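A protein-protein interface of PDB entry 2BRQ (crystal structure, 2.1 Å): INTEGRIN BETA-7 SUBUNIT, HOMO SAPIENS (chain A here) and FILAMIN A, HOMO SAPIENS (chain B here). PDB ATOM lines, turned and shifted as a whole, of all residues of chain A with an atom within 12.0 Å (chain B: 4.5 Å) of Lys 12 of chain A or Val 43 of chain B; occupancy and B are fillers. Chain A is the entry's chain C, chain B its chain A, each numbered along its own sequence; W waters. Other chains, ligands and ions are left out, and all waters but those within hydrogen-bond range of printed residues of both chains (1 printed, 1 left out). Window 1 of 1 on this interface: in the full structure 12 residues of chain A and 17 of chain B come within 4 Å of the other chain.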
ATOM      1  N   PRO A   9       9.364  19.306 -15.654  1.00  0.00           N
ATOM      2  CA  PRO A   9       8.049  18.961 -15.101  1.00  0.00           C
ATOM      3  C   PRO A   9       6.977  18.718 -16.157  1.00  0.00           C
ATOM      4  O   PRO A   9       7.149  19.082 -17.338  1.00  0.00           O
ATOM      5  CB  PRO A   9       7.679  20.196 -14.267  1.00  0.00           C
ATOM      6  CG  PRO A   9       8.973  20.792 -13.871  1.00  0.00           C
ATOM      7  CD  PRO A   9       9.909  20.538 -15.052  1.00  0.00           C
ATOM      8  N   LEU A  10       5.883  18.089 -15.732  1.00  0.00           N
ATOM      9  CA  LEU A  10       4.689  17.984 -16.568  1.00  0.00           C
ATOM     10  C   LEU A  10       3.593  18.981 -16.104  1.00  0.00           C
ATOM     11  O   LEU A  10       3.223  19.004 -14.912  1.00  0.00           O
ATOM     12  CB  LEU A  10       4.180  16.537 -16.558  1.00  0.00           C
ATOM     13  CG  LEU A  10       2.954  16.218 -17.415  1.00  0.00           C
ATOM     14  CD1 LEU A  10       3.285  16.338 -18.898  1.00  0.00           C
ATOM     15  CD2 LEU A  10       2.495  14.816 -17.072  1.00  0.00           C
ATOM     16  N   TYR A  11       3.106  19.805 -17.039  1.00  0.00           N
ATOM     17  CA  TYR A  11       2.215  20.921 -16.728  1.00  0.00           C
ATOM     18  C   TYR A  11       0.812  20.690 -17.255  1.00  0.00           C
ATOM     19  O   TYR A  11       0.631  20.242 -18.375  1.00  0.00           O
ATOM     20  CB  TYR A  11       2.751  22.226 -17.315  1.00  0.00           C
ATOM     21  CG  TYR A  11       4.041  22.711 -16.693  1.00  0.00           C
ATOM     22  CD1 TYR A  11       5.270  22.287 -17.180  1.00  0.00           C
ATOM     23  CD2 TYR A  11       4.028  23.595 -15.618  1.00  0.00           C
ATOM     24  CE1 TYR A  11       6.461  22.733 -16.618  1.00  0.00           C
ATOM     25  CE2 TYR A  11       5.212  24.052 -15.048  1.00  0.00           C
ATOM     26  CZ  TYR A  11       6.427  23.620 -15.555  1.00  0.00           C
ATOM     27  OH  TYR A  11       7.610  24.071 -14.987  1.00  0.00           O
ATOM     28  N   LYS A  12      -0.189  20.979 -16.452  1.00  0.00           N
ATOM     29  CA  LYS A  12      -1.546  20.953 -16.983  1.00  0.00           C
ATOM     30  C   LYS A  12      -2.248  22.258 -16.632  1.00  0.00           C
ATOM     31  O   LYS A  12      -2.095  22.734 -15.509  1.00  0.00           O
ATOM     32  CB  LYS A  12      -2.348  19.764 -16.437  1.00  0.00           C
ATOM     33  CG  LYS A  12      -3.713  19.608 -17.172  1.00  0.00           C
ATOM     34  CD  LYS A  12      -4.549  18.458 -16.636  1.00  0.00           C
ATOM     35  CE  LYS A  12      -5.240  17.745 -17.793  1.00  0.00           C
ATOM     36  NZ  LYS A  12      -5.968  16.542 -17.289  1.00  0.00           N
ATOM     37  N   SER A  13      -2.965  22.844 -17.602  1.00  0.00           N
ATOM     38  CA  SER A  13      -3.872  23.983 -17.354  1.00  0.00           C
ATOM     39  C   SER A  13      -5.228  23.657 -17.922  1.00  0.00           C
ATOM     40  O   SER A  13      -5.311  23.066 -18.988  1.00  0.00           O
ATOM     41  CB  SER A  13      -3.388  25.264 -18.041  1.00  0.00           C
ATOM     42  OG  SER A  13      -2.065  25.600 -17.629  1.00  0.00           O
ATOM     43  N   ALA A  14      -6.274  24.086 -17.211  1.00  0.00           N
ATOM     44  CA  ALA A  14      -7.654  23.809 -17.575  1.00  0.00           C
ATOM     45  C   ALA A  14      -8.497  25.049 -17.280  1.00  0.00           C
ATOM     46  O   ALA A  14      -8.239  25.806 -16.347  1.00  0.00           O
ATOM     47  CB  ALA A  14      -8.210  22.596 -16.787  1.00  0.00           C
ATOM     48  N   ILE A  15      -9.523  25.219 -18.097  1.00  0.00           N
ATOM     49  CA  ILE A  15     -10.536  26.238 -17.836  1.00  0.00           C
ATOM     50  C   ILE A  15     -11.898  25.542 -18.087  1.00  0.00           C
ATOM     51  O   ILE A  15     -12.028  24.760 -19.045  1.00  0.00           O
ATOM     52  CB  ILE A  15     -10.285  27.472 -18.754  1.00  0.00           C
ATOM     53  CG1 ILE A  15     -11.270  28.604 -18.427  1.00  0.00           C
ATOM     54  CG2 ILE A  15     -10.352  27.065 -20.273  1.00  0.00           C
ATOM     55  CD1 ILE A  15     -10.818  29.953 -19.047  1.00  0.00           C
ATOM     56  N   THR A  16     -12.881  25.805 -17.231  1.00  0.00           N
ATOM     57  CA  THR A  16     -14.203  25.188 -17.349  1.00  0.00           C
ATOM     58  C   THR A  16     -15.298  26.242 -17.269  1.00  0.00           C
ATOM     59  O   THR A  16     -15.351  27.032 -16.331  1.00  0.00           O
ATOM     60  CB  THR A  16     -14.428  24.111 -16.263  1.00  0.00           C
ATOM     61  OG1 THR A  16     -13.310  23.197 -16.264  1.00  0.00           O
ATOM     62  CG2 THR A  16     -15.746  23.323 -16.505  1.00  0.00           C
ATOM     63  N   ALA B  42      -8.509  21.563 -21.498  1.00  0.00           N
ATOM     64  CA  ALA B  42      -7.273  21.391 -20.746  1.00  0.00           C
ATOM     65  C   ALA B  42      -6.097  21.159 -21.694  1.00  0.00           C
ATOM     66  O   ALA B  42      -6.257  20.535 -22.738  1.00  0.00           O
ATOM     67  CB  ALA B  42      -7.410  20.244 -19.769  1.00  0.00           C
ATOM     68  N   VAL B  43      -4.932  21.696 -21.341  1.00  0.00           N
ATOM     69  CA  VAL B  43      -3.739  21.525 -22.156  1.00  0.00           C
ATOM     70  C   VAL B  43      -2.672  20.975 -21.221  1.00  0.00           C
ATOM     71  O   VAL B  43      -2.411  21.547 -20.152  1.00  0.00           O
ATOM     72  CB  VAL B  43      -3.258  22.886 -22.758  1.00  0.00           C
ATOM     73  CG1 VAL B  43      -1.944  22.723 -23.529  1.00  0.00           C
ATOM     74  CG2 VAL B  43      -4.365  23.531 -23.631  1.00  0.00           C
ATOM     75  N   GLU B  44      -2.054  19.873 -21.637  1.00  0.00           N
ATOM     76  CA  GLU B  44      -1.057  19.195 -20.805  1.00  0.00           C
ATOM     77  C   GLU B  44       0.200  18.978 -21.649  1.00  0.00           C
ATOM     78  O   GLU B  44       0.110  18.611 -22.826  1.00  0.00           O
ATOM     79  CB  GLU B  44      -1.597  17.867 -20.275  1.00  0.00           C
ATOM     80  CG  GLU B  44      -0.696  17.249 -19.236  1.00  0.00           C
ATOM     81  CD  GLU B  44      -1.120  15.862 -18.813  1.00  0.00           C
ATOM     82  OE1 GLU B  44      -1.237  14.950 -19.663  1.00  0.00           O
ATOM     83  OE2 GLU B  44      -1.271  15.660 -17.608  1.00  0.00           O
ATOM     84  N   GLY B  45       1.356  19.236 -21.048  1.00  0.00           N
ATOM     85  CA  GLY B  45       2.626  19.047 -21.735  1.00  0.00           C
ATOM     86  C   GLY B  45       3.795  19.668 -21.026  1.00  0.00           C
ATOM     87  O   GLY B  45       3.674  20.030 -19.853  1.00  0.00           O
ATOM     88  N   ALA B  49       0.477  26.490 -19.980  1.00  0.00           N
ATOM     89  CA  ALA B  49      -0.426  26.952 -21.015  1.00  0.00           C
ATOM     90  C   ALA B  49      -1.392  27.964 -20.440  1.00  0.00           C
ATOM     91  O   ALA B  49      -1.806  27.877 -19.274  1.00  0.00           O
ATOM     92  CB  ALA B  49      -1.203  25.792 -21.619  1.00  0.00           C
ATOM     93  N   ILE B  51      -5.142  29.589 -21.405  1.00  0.00           N
ATOM     94  CA  ILE B  51      -6.293  29.223 -22.237  1.00  0.00           C
ATOM     95  C   ILE B  51      -7.365  30.280 -22.032  1.00  0.00           C
ATOM     96  O   ILE B  51      -7.587  30.731 -20.909  1.00  0.00           O
ATOM     97  CB  ILE B  51      -6.886  27.824 -21.864  1.00  0.00           C
ATOM     98  CG1 ILE B  51      -5.778  26.794 -21.617  1.00  0.00           C
ATOM     99  CG2 ILE B  51      -7.831  27.335 -22.963  1.00  0.00           C
ATOM    100  CD1 ILE B  51      -6.232  25.468 -20.915  1.00  0.00           C
ATOM    101  N   TYR B  65      -5.304  29.041 -27.038  1.00  0.00           N
ATOM    102  CA  TYR B  65      -4.276  28.750 -26.027  1.00  0.00           C
ATOM    103  C   TYR B  65      -2.860  29.107 -26.517  1.00  0.00           C
ATOM    104  O   TYR B  65      -2.589  29.150 -27.726  1.00  0.00           O
ATOM    105  CB  TYR B  65      -4.338  27.288 -25.534  1.00  0.00           C
ATOM    106  CG  TYR B  65      -3.951  26.274 -26.612  1.00  0.00           C
ATOM    107  CD1 TYR B  65      -4.897  25.783 -27.522  1.00  0.00           C
ATOM    108  CD2 TYR B  65      -2.638  25.812 -26.718  1.00  0.00           C
ATOM    109  CE1 TYR B  65      -4.528  24.859 -28.537  1.00  0.00           C
ATOM    110  CE2 TYR B  65      -2.271  24.869 -27.685  1.00  0.00           C
ATOM    111  CZ  TYR B  65      -3.203  24.407 -28.594  1.00  0.00           C
ATOM    112  OH  TYR B  65      -2.778  23.500 -29.530  1.00  0.00           O
ATOM    113  N   VAL B  67       1.249  28.077 -25.452  1.00  0.00           N
ATOM    114  CA  VAL B  67       2.227  27.337 -24.646  1.00  0.00           C
ATOM    115  C   VAL B  67       3.634  27.918 -24.842  1.00  0.00           C
ATOM    116  O   VAL B  67       3.933  28.523 -25.854  1.00  0.00           O
ATOM    117  CB  VAL B  67       2.262  25.832 -24.935  1.00  0.00           C
ATOM    118  CG1 VAL B  67       0.944  25.157 -24.564  1.00  0.00           C
ATOM    119  CG2 VAL B  67       2.658  25.530 -26.406  1.00  0.00           C
ATOM    120  N   TYR B  73       1.825  18.154 -26.860  1.00  0.00           N
ATOM    121  CA  TYR B  73       0.869  18.538 -25.854  1.00  0.00           C
ATOM    122  C   TYR B  73      -0.407  17.763 -26.087  1.00  0.00           C
ATOM    123  O   TYR B  73      -0.689  17.363 -27.202  1.00  0.00           O
ATOM    124  CB  TYR B  73       0.596  20.046 -25.921  1.00  0.00           C
ATOM    125  CG  TYR B  73       1.765  20.903 -25.445  1.00  0.00           C
ATOM    126  CD1 TYR B  73       2.904  21.091 -26.255  1.00  0.00           C
ATOM    127  CD2 TYR B  73       1.745  21.501 -24.176  1.00  0.00           C
ATOM    128  CE1 TYR B  73       3.971  21.865 -25.817  1.00  0.00           C
ATOM    129  CE2 TYR B  73       2.810  22.279 -23.723  1.00  0.00           C
ATOM    130  CZ  TYR B  73       3.914  22.471 -24.554  1.00  0.00           C
ATOM    131  OH  TYR B  73       4.980  23.243 -24.118  1.00  0.00           O
ATOM    132  N   GLU B  74      -1.167  17.525 -25.028  1.00  0.00           N
ATOM    133  CA  GLU B  74      -2.495  16.917 -25.193  1.00  0.00           C
ATOM    134  C   GLU B  74      -3.537  17.957 -24.861  1.00  0.00           C
ATOM    135  O   GLU B  74      -3.472  18.564 -23.783  1.00  0.00           O
ATOM    136  CB  GLU B  74      -2.690  15.682 -24.309  1.00  0.00           C
ATOM    137  CG  GLU B  74      -2.482  14.343 -25.067  1.00  0.00           C
ATOM    138  CD  GLU B  74      -2.738  13.099 -24.200  1.00  0.00           C
ATOM    139  OE1 GLU B  74      -3.423  13.225 -23.147  1.00  0.00           O
ATOM    140  OE2 GLU B  74      -2.260  11.992 -24.583  1.00  0.00           O
ATOM    141  N   VAL B  75      -4.476  18.180 -25.786  1.00  0.00           N
ATOM    142  CA  VAL B  75      -5.563  19.184 -25.551  1.00  0.00           C
ATOM    143  C   VAL B  75      -6.844  18.360 -25.349  1.00  0.00           C
ATOM    144  O   VAL B  75      -7.278  17.621 -26.230  1.00  0.00           O
ATOM    145  CB  VAL B  75      -5.747  20.201 -26.709  1.00  0.00           C
ATOM    146  CG1 VAL B  75      -6.907  21.215 -26.403  1.00  0.00           C
ATOM    147  CG2 VAL B  75      -4.451  20.983 -27.001  1.00  0.00           C
HETATM  148  O   HOH W   1       0.349  23.082 -19.953  1.00  0.00           O
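The backbone NH (N) of Val 43 of chain B is in hydrogen-bond range of the backbone carbonyl oxygen (O) of Ser 13 of chain A, 2.7 Å away. The side-chain hydroxyl of Ser 13 of chain A lies within hydrogen-bond range of the backbone carbonyl oxygen of Ala 49 of chain B. The backbone carbonyl oxygen (O) of Gly 45 of chain B is in hydrogen-bond range of the backbone NH (N) of Tyr 11 of chain A.
O of Glu 44 of chain B sits at hydrogen-bond distance from N of Glu 74 of chain B, at 2.8 Å.
Among the printed residues, pairs that only touch across the chains: Ser 13 of chain A with Ala 42 of chain B, Tyr 11 of chain A with Glu 44 of chain B, Ser 13 of chain A with Ile 51 of chain B, Lys 12 of chain A with Val 43 of chain B, Ile 15 of chain A with Ile 51 of chain B, Tyr 11 of chain A with Val 43 of chain B, Leu 10 of chain A with Gly 45 of chain B, Lys 12 of chain A with Ala 42 of chain B, Ala 14 of chain A with Ala 42 of chain B, Leu 10 of chain A with Glu 44 of chain B and Ala 14 of chain A with Ile 51 of chain B.
Of the printed residues of chain B, Leu 10 of chain A touches Glu 44 (3.9 Å) and Gly 45 (3.8 Å). Printed residues of chain B within 4 Å of Tyr 11 of chain A: Val 43, Glu 44 and Gly 45. Of chain B, only Ala 42 (3.9 Å) and Val 43 (3.3 Å) come within 4 Å of Lys 12 of chain A. Of the printed residues of chain B, Ser 13 of chain A touches Ala 42 (3.1 Å), Val 43 (2.7 Å), Ala 49 (2.8 Å) and Ile 51 (3.2 Å). Printed residues of chain B within 4 Å of Ile 15 of chain A: Ile 51 (3.7 Å). Thr 16 of chain A touches none of the printed residues of chain B. Ala 42 of chain B touches three residues of chain A. Of chain A, only Tyr 11 (3.8 Å), Lys 12 (3.3 Å) and Ser 13 (2.7 Å) come within 4 Å of Val 43 of chain B. Of chain A, only Leu 10 (3.9 Å) and Tyr 11 (3.1 Å) come within 4 Å of Glu 44 of chain B. Gly 45 of chain B touches just these residues of chain A: Leu 10 and Tyr 11. Tyr 65 of chain B touches none of the printed residues of chain A. No residue of chain A comes within 4 Å of Tyr 73 of chain B. Glu 74 of chain B touches none of the printed residues of chain A. No residue of chain A comes within 4 Å of Val 75 of chain B.
Of the 11 printed residues of chain B, 6 touch a printed residue of chain A. Hydrophobic or aromatic side chains of chain A within 4 Å of the printed part of chain B: Leu 10, Tyr 11, Ala 14 and Ile 15. Among the printed residues, 14 pairs touch across the chains. Among the printed residues, no Asp or Glu carboxylate lies within 4 Å of a Lys or Arg side-chain nitrogen of the other chain.
Water W1 lies within hydrogen-bond range of the backbone carbonyl oxygen of Val 43 of chain B (3.2 Å), the backbone carbonyl oxygen of Tyr 11 of chain A (3.3 Å) and the backbone NH of Ala 49 of chain B (3.4 Å).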
